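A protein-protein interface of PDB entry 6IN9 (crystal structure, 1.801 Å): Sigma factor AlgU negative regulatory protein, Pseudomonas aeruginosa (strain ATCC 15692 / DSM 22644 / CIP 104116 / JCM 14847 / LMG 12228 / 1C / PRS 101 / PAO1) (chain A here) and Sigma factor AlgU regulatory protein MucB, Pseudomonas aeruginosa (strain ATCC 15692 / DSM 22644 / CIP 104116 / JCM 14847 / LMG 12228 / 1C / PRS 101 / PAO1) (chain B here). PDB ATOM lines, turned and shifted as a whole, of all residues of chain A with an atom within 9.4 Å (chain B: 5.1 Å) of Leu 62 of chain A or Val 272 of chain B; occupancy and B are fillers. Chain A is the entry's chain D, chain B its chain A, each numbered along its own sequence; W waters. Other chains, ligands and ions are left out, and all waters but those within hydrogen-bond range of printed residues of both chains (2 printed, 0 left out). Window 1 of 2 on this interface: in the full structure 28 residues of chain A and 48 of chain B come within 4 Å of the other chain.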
ATOM      1  N   GLN A  41      -0.130   7.642  34.178  1.00  0.00           N
ATOM      2  CA  GLN A  41      -0.856   8.848  33.800  1.00  0.00           C
ATOM      3  C   GLN A  41      -2.038   9.092  34.734  1.00  0.00           C
ATOM      4  O   GLN A  41      -2.948   9.860  34.408  1.00  0.00           O
ATOM      5  CB  GLN A  41      -1.365   8.748  32.358  1.00  0.00           C
ATOM      6  CG  GLN A  41      -0.446   8.026  31.394  1.00  0.00           C
ATOM      7  CD  GLN A  41      -0.997   6.672  30.977  1.00  0.00           C
ATOM      8  OE1 GLN A  41      -1.950   6.165  31.573  1.00  0.00           O
ATOM      9  NE2 GLN A  41      -0.402   6.084  29.945  1.00  0.00           N
ATOM     10  N   VAL A  42      -2.025   8.439  35.890  1.00  0.00           N
ATOM     11  CA  VAL A  42      -3.221   8.349  36.721  1.00  0.00           C
ATOM     12  C   VAL A  42      -3.392   9.640  37.508  1.00  0.00           C
ATOM     13  O   VAL A  42      -2.539  10.002  38.325  1.00  0.00           O
ATOM     14  CB  VAL A  42      -3.157   7.133  37.654  1.00  0.00           C
ATOM     15  CG1 VAL A  42      -4.366   7.120  38.585  1.00  0.00           C
ATOM     16  CG2 VAL A  42      -3.098   5.854  36.828  1.00  0.00           C
ATOM     17  N   HIS A  54      -4.820   2.574  41.835  1.00  0.00           N
ATOM     18  CA  HIS A  54      -5.236   2.780  40.453  1.00  0.00           C
ATOM     19  C   HIS A  54      -4.095   2.571  39.459  1.00  0.00           C
ATOM     20  O   HIS A  54      -4.344   2.131  38.326  1.00  0.00           O
ATOM     21  CB  HIS A  54      -5.823   4.179  40.288  1.00  0.00           C
ATOM     22  CG  HIS A  54      -7.214   4.316  40.826  1.00  0.00           C
ATOM     23  ND1 HIS A  54      -8.295   3.680  40.252  1.00  0.00           N
ATOM     24  CD2 HIS A  54      -7.707   5.043  41.858  1.00  0.00           C
ATOM     25  CE1 HIS A  54      -9.394   3.992  40.920  1.00  0.00           C
ATOM     26  NE2 HIS A  54      -9.066   4.826  41.893  1.00  0.00           N
ATOM     27  N   GLN A  56      -1.879   0.357  39.265  1.00  0.00           N
ATOM     28  CA  GLN A  56      -1.677  -1.038  38.899  1.00  0.00           C
ATOM     29  C   GLN A  56      -2.772  -1.588  37.996  1.00  0.00           C
ATOM     30  O   GLN A  56      -2.653  -2.728  37.520  1.00  0.00           O
ATOM     31  CB  GLN A  56      -1.602  -1.899  40.158  1.00  0.00           C
ATOM     32  CG  GLN A  56      -0.343  -1.713  40.960  1.00  0.00           C
ATOM     33  CD  GLN A  56      -0.259  -2.719  42.083  1.00  0.00           C
ATOM     34  OE1 GLN A  56      -0.802  -2.500  43.162  1.00  0.00           O
ATOM     35  NE2 GLN A  56       0.410  -3.840  41.829  1.00  0.00           N
ATOM     36  N   ARG A  57      -3.835  -0.824  37.771  1.00  0.00           N
ATOM     37  CA  ARG A  57      -5.021  -1.295  37.070  1.00  0.00           C
ATOM     38  C   ARG A  57      -5.345  -0.462  35.842  1.00  0.00           C
ATOM     39  O   ARG A  57      -5.509  -1.019  34.750  1.00  0.00           O
ATOM     40  CB  ARG A  57      -6.225  -1.288  38.032  1.00  0.00           C
ATOM     41  CG  ARG A  57      -6.125  -2.359  39.119  1.00  0.00           C
ATOM     42  CD  ARG A  57      -6.978  -2.021  40.303  1.00  0.00           C
ATOM     43  NE  ARG A  57      -7.001  -3.111  41.277  1.00  0.00           N
ATOM     44  CZ  ARG A  57      -6.146  -3.245  42.287  1.00  0.00           C
ATOM     45  NH1 ARG A  57      -5.176  -2.357  42.481  1.00  0.00           N
ATOM     46  NH2 ARG A  57      -6.267  -4.272  43.117  1.00  0.00           N
ATOM     47  N   LEU A  58      -5.457   0.861  35.999  1.00  0.00           N
ATOM     48  CA  LEU A  58      -5.906   1.710  34.895  1.00  0.00           C
ATOM     49  C   LEU A  58      -5.069   1.575  33.630  1.00  0.00           C
ATOM     50  O   LEU A  58      -5.667   1.507  32.541  1.00  0.00           O
ATOM     51  CB  LEU A  58      -5.931   3.183  35.319  1.00  0.00           C
ATOM     52  CG  LEU A  58      -6.975   3.642  36.317  1.00  0.00           C
ATOM     53  CD1 LEU A  58      -6.961   5.164  36.363  1.00  0.00           C
ATOM     54  CD2 LEU A  58      -8.331   3.111  35.912  1.00  0.00           C
ATOM     55  N   PRO A  59      -3.734   1.563  33.678  1.00  0.00           N
ATOM     56  CA  PRO A  59      -2.979   1.402  32.427  1.00  0.00           C
ATOM     57  C   PRO A  59      -3.310   0.118  31.709  1.00  0.00           C
ATOM     58  O   PRO A  59      -3.323   0.099  30.472  1.00  0.00           O
ATOM     59  CB  PRO A  59      -1.512   1.426  32.896  1.00  0.00           C
ATOM     60  CG  PRO A  59      -1.551   2.215  34.167  1.00  0.00           C
ATOM     61  CD  PRO A  59      -2.833   1.782  34.826  1.00  0.00           C
ATOM     62  N   ILE A  60      -3.616  -0.952  32.455  1.00  0.00           N
ATOM     63  CA  ILE A  60      -3.922  -2.238  31.842  1.00  0.00           C
ATOM     64  C   ILE A  60      -5.294  -2.218  31.173  1.00  0.00           C
ATOM     65  O   ILE A  60      -5.465  -2.765  30.076  1.00  0.00           O
ATOM     66  CB  ILE A  60      -3.831  -3.359  32.895  1.00  0.00           C
ATOM     67  CG1 ILE A  60      -2.383  -3.505  33.382  1.00  0.00           C
ATOM     68  CG2 ILE A  60      -4.398  -4.658  32.331  1.00  0.00           C
ATOM     69  CD1 ILE A  60      -1.471  -4.138  32.366  1.00  0.00           C
ATOM     70  N   TYR A  61      -6.303  -1.650  31.851  1.00  0.00           N
ATOM     71  CA  TYR A  61      -7.637  -1.556  31.262  1.00  0.00           C
ATOM     72  C   TYR A  61      -7.627  -0.646  30.039  1.00  0.00           C
ATOM     73  O   TYR A  61      -8.326  -0.915  29.054  1.00  0.00           O
ATOM     74  CB  TYR A  61      -8.641  -1.055  32.307  1.00  0.00           C
ATOM     75  CG  TYR A  61      -8.778  -1.999  33.499  1.00  0.00           C
ATOM     76  CD1 TYR A  61      -8.536  -3.362  33.356  1.00  0.00           C
ATOM     77  CD2 TYR A  61      -9.136  -1.526  34.755  1.00  0.00           C
ATOM     78  CE1 TYR A  61      -8.655  -4.242  34.443  1.00  0.00           C
ATOM     79  CE2 TYR A  61      -9.273  -2.399  35.844  1.00  0.00           C
ATOM     80  CZ  TYR A  61      -9.026  -3.747  35.681  1.00  0.00           C
ATOM     81  OH  TYR A  61      -9.150  -4.614  36.767  1.00  0.00           O
ATOM     82  N   LEU A  62      -6.856   0.446  30.093  1.00  0.00           N
ATOM     83  CA  LEU A  62      -6.680   1.301  28.915  1.00  0.00           C
ATOM     84  C   LEU A  62      -6.134   0.501  27.738  1.00  0.00           C
ATOM     85  O   LEU A  62      -6.696   0.523  26.635  1.00  0.00           O
ATOM     86  CB  LEU A  62      -5.745   2.461  29.243  1.00  0.00           C
ATOM     87  CG  LEU A  62      -5.336   3.374  28.081  1.00  0.00           C
ATOM     88  CD1 LEU A  62      -6.526   4.138  27.576  1.00  0.00           C
ATOM     89  CD2 LEU A  62      -4.243   4.329  28.524  1.00  0.00           C
ATOM     90  N   ARG A  63      -5.041  -0.230  27.961  1.00  0.00           N
ATOM     91  CA  ARG A  63      -4.473  -1.037  26.887  1.00  0.00           C
ATOM     92  C   ARG A  63      -5.483  -2.043  26.357  1.00  0.00           C
ATOM     93  O   ARG A  63      -5.578  -2.250  25.141  1.00  0.00           O
ATOM     94  CB  ARG A  63      -3.208  -1.759  27.358  1.00  0.00           C
ATOM     95  CG  ARG A  63      -1.991  -0.884  27.497  1.00  0.00           C
ATOM     96  CD  ARG A  63      -0.754  -1.702  27.938  1.00  0.00           C
ATOM     97  NE  ARG A  63      -0.165  -2.501  26.860  1.00  0.00           N
ATOM     98  CZ  ARG A  63       0.687  -2.021  25.958  1.00  0.00           C
ATOM     99  NH1 ARG A  63       1.191  -2.811  25.017  1.00  0.00           N
ATOM    100  NH2 ARG A  63       1.024  -0.739  25.983  1.00  0.00           N
ATOM    101  N   GLN A  64      -6.245  -2.691  27.245  1.00  0.00           N
ATOM    102  CA  GLN A  64      -7.220  -3.657  26.759  1.00  0.00           C
ATOM    103  C   GLN A  64      -8.249  -2.995  25.860  1.00  0.00           C
ATOM    104  O   GLN A  64      -8.591  -3.530  24.800  1.00  0.00           O
ATOM    105  CB  GLN A  64      -7.929  -4.358  27.914  1.00  0.00           C
ATOM    106  CG  GLN A  64      -8.942  -5.368  27.413  1.00  0.00           C
ATOM    107  CD  GLN A  64      -9.829  -5.908  28.524  1.00  0.00           C
ATOM    108  OE1 GLN A  64      -9.355  -6.245  29.604  1.00  0.00           O
ATOM    109  NE2 GLN A  64     -11.118  -5.964  28.266  1.00  0.00           N
ATOM    110  N   HIS A  65      -8.768  -1.836  26.270  1.00  0.00           N
ATOM    111  CA  HIS A  65      -9.782  -1.192  25.447  1.00  0.00           C
ATOM    112  C   HIS A  65      -9.225  -0.870  24.070  1.00  0.00           C
ATOM    113  O   HIS A  65      -9.850  -1.161  23.052  1.00  0.00           O
ATOM    114  CB  HIS A  65     -10.293   0.088  26.087  1.00  0.00           C
ATOM    115  CG  HIS A  65     -11.139   0.899  25.148  1.00  0.00           C
ATOM    116  ND1 HIS A  65     -12.419   0.529  24.803  1.00  0.00           N
ATOM    117  CD2 HIS A  65     -10.861   2.014  24.429  1.00  0.00           C
ATOM    118  CE1 HIS A  65     -12.911   1.402  23.938  1.00  0.00           C
ATOM    119  NE2 HIS A  65     -11.980   2.305  23.685  1.00  0.00           N
ATOM    120  N   VAL A  66      -8.031  -0.290  24.027  1.00  0.00           N
ATOM    121  CA  VAL A  66      -7.525   0.180  22.743  1.00  0.00           C
ATOM    122  C   VAL A  66      -7.135  -0.999  21.866  1.00  0.00           C
ATOM    123  O   VAL A  66      -7.400  -1.001  20.660  1.00  0.00           O
ATOM    124  CB  VAL A  66      -6.364   1.160  22.958  1.00  0.00           C
ATOM    125  CG1 VAL A  66      -5.810   1.604  21.617  1.00  0.00           C
ATOM    126  CG2 VAL A  66      -6.855   2.372  23.757  1.00  0.00           C
ATOM    127  N   GLN A  67      -6.529  -2.037  22.460  1.00  0.00           N
ATOM    128  CA  GLN A  67      -6.100  -3.187  21.660  1.00  0.00           C
ATOM    129  C   GLN A  67      -7.285  -3.976  21.131  1.00  0.00           C
ATOM    130  O   GLN A  67      -7.290  -4.399  19.966  1.00  0.00           O
ATOM    131  CB  GLN A  67      -5.191  -4.102  22.486  1.00  0.00           C
ATOM    132  CG  GLN A  67      -3.805  -3.553  22.689  1.00  0.00           C
ATOM    133  CD  GLN A  67      -2.933  -4.458  23.534  1.00  0.00           C
ATOM    134  OE1 GLN A  67      -3.367  -5.524  23.982  1.00  0.00           O
ATOM    135  NE2 GLN A  67      -1.702  -4.037  23.758  1.00  0.00           N
ATOM    136  N   GLN A  68      -8.288  -4.224  21.975  1.00  0.00           N
ATOM    137  CA  GLN A  68      -9.444  -4.964  21.493  1.00  0.00           C
ATOM    138  C   GLN A  68     -10.190  -4.178  20.426  1.00  0.00           C
ATOM    139  O   GLN A  68     -10.708  -4.771  19.477  1.00  0.00           O
ATOM    140  CB  GLN A  68     -10.364  -5.330  22.670  1.00  0.00           C
ATOM    141  CG  GLN A  68      -9.700  -6.298  23.638  1.00  0.00           C
ATOM    142  CD  GLN A  68     -10.655  -6.874  24.689  1.00  0.00           C
ATOM    143  OE1 GLN A  68     -11.603  -6.213  25.127  1.00  0.00           O
ATOM    144  NE2 GLN A  68     -10.409  -8.117  25.083  1.00  0.00           N
ATOM    145  N   SER A  69     -10.233  -2.848  20.542  1.00  0.00           N
ATOM    146  CA  SER A  69     -10.921  -2.058  19.522  1.00  0.00           C
ATOM    147  C   SER A  69     -10.209  -2.147  18.181  1.00  0.00           C
ATOM    148  O   SER A  69     -10.839  -1.984  17.131  1.00  0.00           O
ATOM    149  CB  SER A  69     -11.020  -0.597  19.963  1.00  0.00           C
ATOM    150  OG  SER A  69     -11.733  -0.499  21.190  1.00  0.00           O
ATOM    151  N   ALA A  70      -8.902  -2.398  18.202  1.00  0.00           N
ATOM    152  CA  ALA A  70      -8.117  -2.531  16.983  1.00  0.00           C
ATOM    153  C   ALA A  70      -8.325  -3.877  16.299  1.00  0.00           C
ATOM    154  O   ALA A  70      -8.167  -3.967  15.082  1.00  0.00           O
ATOM    155  CB  ALA A  70      -6.631  -2.332  17.297  1.00  0.00           C
ATOM    156  N   ARG A  82      -4.101   3.651  16.794  1.00  0.00           N
ATOM    157  CA  ARG A  82      -4.242   4.010  18.204  1.00  0.00           C
ATOM    158  C   ARG A  82      -3.553   2.990  19.101  1.00  0.00           C
ATOM    159  O   ARG A  82      -2.851   3.359  20.052  1.00  0.00           O
ATOM    160  CB  ARG A  82      -5.727   4.123  18.584  1.00  0.00           C
ATOM    161  CG  ARG A  82      -6.500   5.198  17.857  1.00  0.00           C
ATOM    162  CD  ARG A  82      -8.002   5.109  18.258  1.00  0.00           C
ATOM    163  NE  ARG A  82      -8.761   6.218  17.678  1.00  0.00           N
ATOM    164  CZ  ARG A  82     -10.065   6.173  17.443  1.00  0.00           C
ATOM    165  NH1 ARG A  82     -10.761   5.068  17.753  1.00  0.00           N
ATOM    166  NH2 ARG A  82     -10.674   7.232  16.919  1.00  0.00           N
ATOM    167  N   ALA A  83      -3.737   1.699  18.809  1.00  0.00           N
ATOM    168  CA  ALA A  83      -3.047   0.658  19.565  1.00  0.00           C
ATOM    169  C   ALA A  83      -1.543   0.785  19.419  1.00  0.00           C
ATOM    170  O   ALA A  83      -0.795   0.654  20.400  1.00  0.00           O
ATOM    171  CB  ALA A  83      -3.513  -0.726  19.105  1.00  0.00           C
ATOM    172  N   SER A  85       0.148   3.400  19.022  1.00  0.00           N
ATOM    173  CA  SER A  85       0.652   4.589  19.699  1.00  0.00           C
ATOM    174  C   SER A  85       0.955   4.340  21.170  1.00  0.00           C
ATOM    175  O   SER A  85       1.636   5.160  21.791  1.00  0.00           O
ATOM    176  CB  SER A  85      -0.340   5.747  19.579  1.00  0.00           C
ATOM    177  OG  SER A  85      -1.401   5.594  20.519  1.00  0.00           O
ATOM    178  N   LEU A  86       0.486   3.236  21.739  1.00  0.00           N
ATOM    179  CA  LEU A  86       0.732   2.976  23.152  1.00  0.00           C
ATOM    180  C   LEU A  86       2.198   2.601  23.390  1.00  0.00           C
ATOM    181  O   LEU A  86       2.907   2.151  22.486  1.00  0.00           O
ATOM    182  CB  LEU A  86      -0.185   1.865  23.659  1.00  0.00           C
ATOM    183  CG  LEU A  86      -1.675   2.072  23.400  1.00  0.00           C
ATOM    184  CD1 LEU A  86      -2.472   0.939  24.004  1.00  0.00           C
ATOM    185  CD2 LEU A  86      -2.110   3.395  23.976  1.00  0.00           C
ATOM    186  N   GLU A  87       2.642   2.790  24.634  1.00  0.00           N
ATOM    187  CA  GLU A  87       4.051   2.612  25.020  1.00  0.00           C
ATOM    188  C   GLU A  87       4.989   3.337  24.054  1.00  0.00           C
ATOM    189  O   GLU A  87       5.283   4.522  24.224  1.00  0.00           O
ATOM    190  CB  GLU A  87       4.428   1.120  25.096  1.00  0.00           C
ATOM    191  CG  GLU A  87       5.892   0.827  24.736  1.00  0.00           C
ATOM    192  CD  GLU A  87       6.188  -0.651  24.492  1.00  0.00           C
ATOM    193  OE1 GLU A  87       5.336  -1.347  23.901  1.00  0.00           O
ATOM    194  OE2 GLU A  87       7.286  -1.115  24.874  1.00  0.00           O
ATOM    195  N   ARG B 230     -16.474   4.002  20.606  1.00  0.00           N
ATOM    196  CA  ARG B 230     -16.519   2.837  21.474  1.00  0.00           C
ATOM    197  C   ARG B 230     -16.071   3.230  22.872  1.00  0.00           C
ATOM    198  O   ARG B 230     -15.256   4.136  23.041  1.00  0.00           O
ATOM    199  CB  ARG B 230     -15.622   1.706  20.962  1.00  0.00           C
ATOM    200  CG  ARG B 230     -15.992   1.211  19.580  1.00  0.00           C
ATOM    201  CD  ARG B 230     -15.419  -0.173  19.308  1.00  0.00           C
ATOM    202  NE  ARG B 230     -15.485  -0.514  17.893  1.00  0.00           N
ATOM    203  CZ  ARG B 230     -16.502  -1.153  17.321  1.00  0.00           C
ATOM    204  NH1 ARG B 230     -17.568  -1.509  18.035  1.00  0.00           N
ATOM    205  NH2 ARG B 230     -16.466  -1.419  16.021  1.00  0.00           N
ATOM    206  N   PHE B 231     -16.630   2.558  23.878  1.00  0.00           N
ATOM    207  CA  PHE B 231     -16.057   2.621  25.218  1.00  0.00           C
ATOM    208  C   PHE B 231     -16.254   1.273  25.898  1.00  0.00           C
ATOM    209  O   PHE B 231     -17.118   0.480  25.513  1.00  0.00           O
ATOM    210  CB  PHE B 231     -16.633   3.783  26.060  1.00  0.00           C
ATOM    211  CG  PHE B 231     -18.119   3.721  26.308  1.00  0.00           C
ATOM    212  CD1 PHE B 231     -18.636   2.937  27.338  1.00  0.00           C
ATOM    213  CD2 PHE B 231     -18.992   4.496  25.551  1.00  0.00           C
ATOM    214  CE1 PHE B 231     -20.007   2.910  27.591  1.00  0.00           C
ATOM    215  CE2 PHE B 231     -20.366   4.466  25.799  1.00  0.00           C
ATOM    216  CZ  PHE B 231     -20.864   3.674  26.820  1.00  0.00           C
ATOM    217  N   SER B 232     -15.415   1.019  26.896  1.00  0.00           N
ATOM    218  CA  SER B 232     -15.394  -0.227  27.652  1.00  0.00           C
ATOM    219  C   SER B 232     -15.609   0.086  29.127  1.00  0.00           C
ATOM    220  O   SER B 232     -15.158   1.118  29.629  1.00  0.00           O
ATOM    221  CB  SER B 232     -14.063  -0.982  27.485  1.00  0.00           C
ATOM    222  OG  SER B 232     -13.818  -1.359  26.122  1.00  0.00           O
ATOM    223  N   PHE B 234     -15.281  -1.601  33.079  1.00  0.00           N
ATOM    224  CA  PHE B 234     -14.642  -2.622  33.903  1.00  0.00           C
ATOM    225  C   PHE B 234     -15.219  -2.482  35.294  1.00  0.00           C
ATOM    226  O   PHE B 234     -15.306  -1.361  35.799  1.00  0.00           O
ATOM    227  CB  PHE B 234     -13.130  -2.438  33.976  1.00  0.00           C
ATOM    228  CG  PHE B 234     -12.461  -2.443  32.633  1.00  0.00           C
ATOM    229  CD1 PHE B 234     -12.471  -1.312  31.837  1.00  0.00           C
ATOM    230  CD2 PHE B 234     -11.859  -3.592  32.159  1.00  0.00           C
ATOM    231  CE1 PHE B 234     -11.888  -1.323  30.591  1.00  0.00           C
ATOM    232  CE2 PHE B 234     -11.262  -3.607  30.916  1.00  0.00           C
ATOM    233  CZ  PHE B 234     -11.277  -2.479  30.132  1.00  0.00           C
ATOM    234  N   LEU B 250      -5.534   9.789  27.473  1.00  0.00           N
ATOM    235  CA  LEU B 250      -4.477   9.457  26.516  1.00  0.00           C
ATOM    236  C   LEU B 250      -5.009   9.825  25.136  1.00  0.00           C
ATOM    237  O   LEU B 250      -5.725   9.039  24.506  1.00  0.00           O
ATOM    238  CB  LEU B 250      -4.086   7.990  26.598  1.00  0.00           C
ATOM    239  CG  LEU B 250      -2.718   7.641  26.003  1.00  0.00           C
ATOM    240  CD1 LEU B 250      -1.592   8.281  26.791  1.00  0.00           C
ATOM    241  CD2 LEU B 250      -2.541   6.161  25.952  1.00  0.00           C
ATOM    242  N   THR B 253      -8.681   9.202  24.212  1.00  0.00           N
ATOM    243  CA  THR B 253      -9.213   8.168  25.094  1.00  0.00           C
ATOM    244  C   THR B 253      -9.222   8.679  26.530  1.00  0.00           C
ATOM    245  O   THR B 253      -8.161   8.936  27.109  1.00  0.00           O
ATOM    246  CB  THR B 253      -8.385   6.888  25.000  1.00  0.00           C
ATOM    247  OG1 THR B 253      -8.268   6.489  23.628  1.00  0.00           O
ATOM    248  CG2 THR B 253      -9.066   5.761  25.780  1.00  0.00           C
ATOM    249  N   VAL B 254     -10.404   8.785  27.105  1.00  0.00           N
ATOM    250  CA  VAL B 254     -10.565   9.171  28.502  1.00  0.00           C
ATOM    251  C   VAL B 254     -10.666   7.910  29.352  1.00  0.00           C
ATOM    252  O   VAL B 254     -11.097   6.849  28.883  1.00  0.00           O
ATOM    253  CB  VAL B 254     -11.802  10.080  28.684  1.00  0.00           C
ATOM    254  CG1 VAL B 254     -13.111   9.265  28.598  1.00  0.00           C
ATOM    255  CG2 VAL B 254     -11.710  10.857  30.003  1.00  0.00           C
ATOM    256  N   VAL B 255     -10.218   8.020  30.604  1.00  0.00           N
ATOM    257  CA  VAL B 255     -10.347   6.969  31.616  1.00  0.00           C
ATOM    258  C   VAL B 255     -10.932   7.620  32.852  1.00  0.00           C
ATOM    259  O   VAL B 255     -10.353   8.582  33.363  1.00  0.00           O
ATOM    260  CB  VAL B 255      -8.993   6.332  31.978  1.00  0.00           C
ATOM    261  CG1 VAL B 255      -9.202   5.157  32.936  1.00  0.00           C
ATOM    262  CG2 VAL B 255      -8.207   5.934  30.743  1.00  0.00           C
ATOM    263  N   THR B 270     -14.671   1.391  36.056  1.00  0.00           N
ATOM    264  CA  THR B 270     -13.786   2.149  35.175  1.00  0.00           C
ATOM    265  C   THR B 270     -14.372   2.191  33.766  1.00  0.00           C
ATOM    266  O   THR B 270     -14.780   1.157  33.225  1.00  0.00           O
ATOM    267  CB  THR B 270     -12.376   1.547  35.158  1.00  0.00           C
ATOM    268  OG1 THR B 270     -11.820   1.607  36.473  1.00  0.00           O
ATOM    269  CG2 THR B 270     -11.456   2.332  34.216  1.00  0.00           C
ATOM    270  N   VAL B 271     -14.462   3.391  33.192  1.00  0.00           N
ATOM    271  CA  VAL B 271     -14.935   3.556  31.823  1.00  0.00           C
ATOM    272  C   VAL B 271     -13.780   4.118  31.012  1.00  0.00           C
ATOM    273  O   VAL B 271     -13.181   5.133  31.399  1.00  0.00           O
ATOM    274  CB  VAL B 271     -16.177   4.467  31.732  1.00  0.00           C
ATOM    275  CG1 VAL B 271     -16.569   4.656  30.275  1.00  0.00           C
ATOM    276  CG2 VAL B 271     -17.357   3.811  32.449  1.00  0.00           C
ATOM    277  N   VAL B 272     -13.481   3.469  29.886  1.00  0.00           N
ATOM    278  CA  VAL B 272     -12.382   3.862  29.008  1.00  0.00           C
ATOM    279  C   VAL B 272     -12.947   3.988  27.602  1.00  0.00           C
ATOM    280  O   VAL B 272     -13.541   3.032  27.095  1.00  0.00           O
ATOM    281  CB  VAL B 272     -11.238   2.827  28.999  1.00  0.00           C
ATOM    282  CG1 VAL B 272     -10.122   3.265  28.040  1.00  0.00           C
ATOM    283  CG2 VAL B 272     -10.668   2.573  30.396  1.00  0.00           C
ATOM    284  N   GLY B 273     -12.732   5.124  26.953  1.00  0.00           N
ATOM    285  CA  GLY B 273     -13.096   5.163  25.552  1.00  0.00           C
ATOM    286  C   GLY B 273     -12.976   6.537  24.936  1.00  0.00           C
ATOM    287  O   GLY B 273     -12.561   7.508  25.569  1.00  0.00           O
ATOM    288  N   GLU B 274     -13.365   6.589  23.666  1.00  0.00           N
ATOM    289  CA  GLU B 274     -13.209   7.796  22.856  1.00  0.00           C
ATOM    290  C   GLU B 274     -14.498   8.610  22.876  1.00  0.00           C
ATOM    291  O   GLU B 274     -15.177   8.814  21.865  1.00  0.00           O
ATOM    292  CB  GLU B 274     -12.776   7.423  21.440  1.00  0.00           C
ATOM    293  CG  GLU B 274     -11.368   6.755  21.381  1.00  0.00           C
ATOM    294  CD  GLU B 274     -11.335   5.329  21.982  1.00  0.00           C
ATOM    295  OE1 GLU B 274     -10.439   5.023  22.801  1.00  0.00           O
ATOM    296  OE2 GLU B 274     -12.209   4.516  21.641  1.00  0.00           O
HETATM  297  O   HOH W   1     -12.452  -3.646  25.717  1.00  0.00           O
HETATM  298  O   HOH W   2      -9.215   1.437  38.489  1.00  0.00           O
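The side-chain hydroxyl (OG) of Ser 232 of chain B lies within hydrogen-bond range of a ring nitrogen (ND1) of His 65 of chain A, 2.7 Å away.
NE2 of His 65 of chain A is in hydrogen-bond range of OE2 of Glu 274 of chain B (3.0 Å).
Of the printed residues of chain B, Leu 62 of chain A touches Leu 250, Thr 253 and Val 272.
Gln 68 of chain A touches none of the printed residues of chain B.
Glu 87 of chain A touches none of the printed residues of chain B.
Ser 232 of chain B touches just one residue of chain A: His 65 (2.7 Å).
Of the printed residues of chain A, Phe 234 of chain B touches Tyr 61 (3.5 Å) and Gln 64 (3.5 Å).
Of the printed residues of chain A, Thr 253 of chain B touches Leu 62 (3.5 Å).
Printed residues of chain A within 4 Å of Val 255 of chain B: Leu 58.
No residue of chain A comes within 4 Å of Val 271 of chain B.
Val 272 of chain B touches just these residues of chain A: Leu 62 and His 65.
Printed residues of chain A within 4 Å of Gly 273 of chain B: His 65 (3.6 Å).
The nearest printed residue of chain B that does not touch Leu 62 of chain A is Val 255 of chain B (4.01 Å).
The nearest residue of chain A that does not touch Val 272 of chain B is Tyr 61 of chain A (4.4 Å).
Water W1 lies within hydrogen-bond range of the side-chain hydroxyl of Ser 232 of chain B and the side-chain amide oxygen of Gln 68 of chain A.
Water W2 lies within hydrogen-bond range of ND1 of His 54 of chain A and OG1 of Thr 270 of chain B.
Among the printed residues, merely in contact across the chains: Leu 86 of chain A with Leu 250 of chain B (3.4 Å), Leu 62 of chain A with Thr 253 of chain B (3.5 Å), Tyr 61 of chain A with Phe 234 of chain B (3.5 Å), Gln 64 of chain A with Phe 234 of chain B (3.5 Å), His 65 of chain A with Val 272 of chain B (3.6 Å), Leu 62 of chain A with Leu 250 of chain B (3.6 Å), His 65 of chain A with Gly 273 of chain B (3.6 Å), His 65 of chain A with Phe 231 of chain B (3.6 Å), Leu 58 of chain A with Thr 270 of chain B (3.6 Å), His 65 of chain A with Arg 230 of chain B (3.7 Å), Leu 58 of chain A with Val 255 of chain B (3.7 Å) and Leu 62 of chain A with Val 272 of chain B (3.7 Å).
Of the 23 printed residues of chain A, 6 touch a printed residue of chain B.
Among the printed residues, no Asp or Glu carboxylate lies within 4 Å of a Lys or Arg side-chain nitrogen of the other chain.
The backbone carbonyl oxygen (O) of Arg 230 of chain B lies within hydrogen-bond range of the backbone NH (N) of Glu 274 of chain B, at 3.2 Å.
The backbone NH (N) of Phe 234 of chain B sits at hydrogen-bond distance from the backbone carbonyl oxygen (O) of Thr 270 of chain B (2.8 Å).
The side-chain hydroxyl (OG1) of Thr 253 of chain B sits at hydrogen-bond distance from the side-chain carboxylate (OE1) of Glu 274 of chain B (2.7 Å).
N of Val 254 of chain B sits at hydrogen-bond distance from O of Gly 273 of chain B (2.9 Å).
The side-chain amide nitrogen of Gln 64 of chain A lies within hydrogen-bond range of the side-chain amide oxygen of Gln 68 of chain A, 3.2 Å away.
OG of Ser 69 of chain A lies within hydrogen-bond range of O of His 65 of chain A (2.7 Å).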
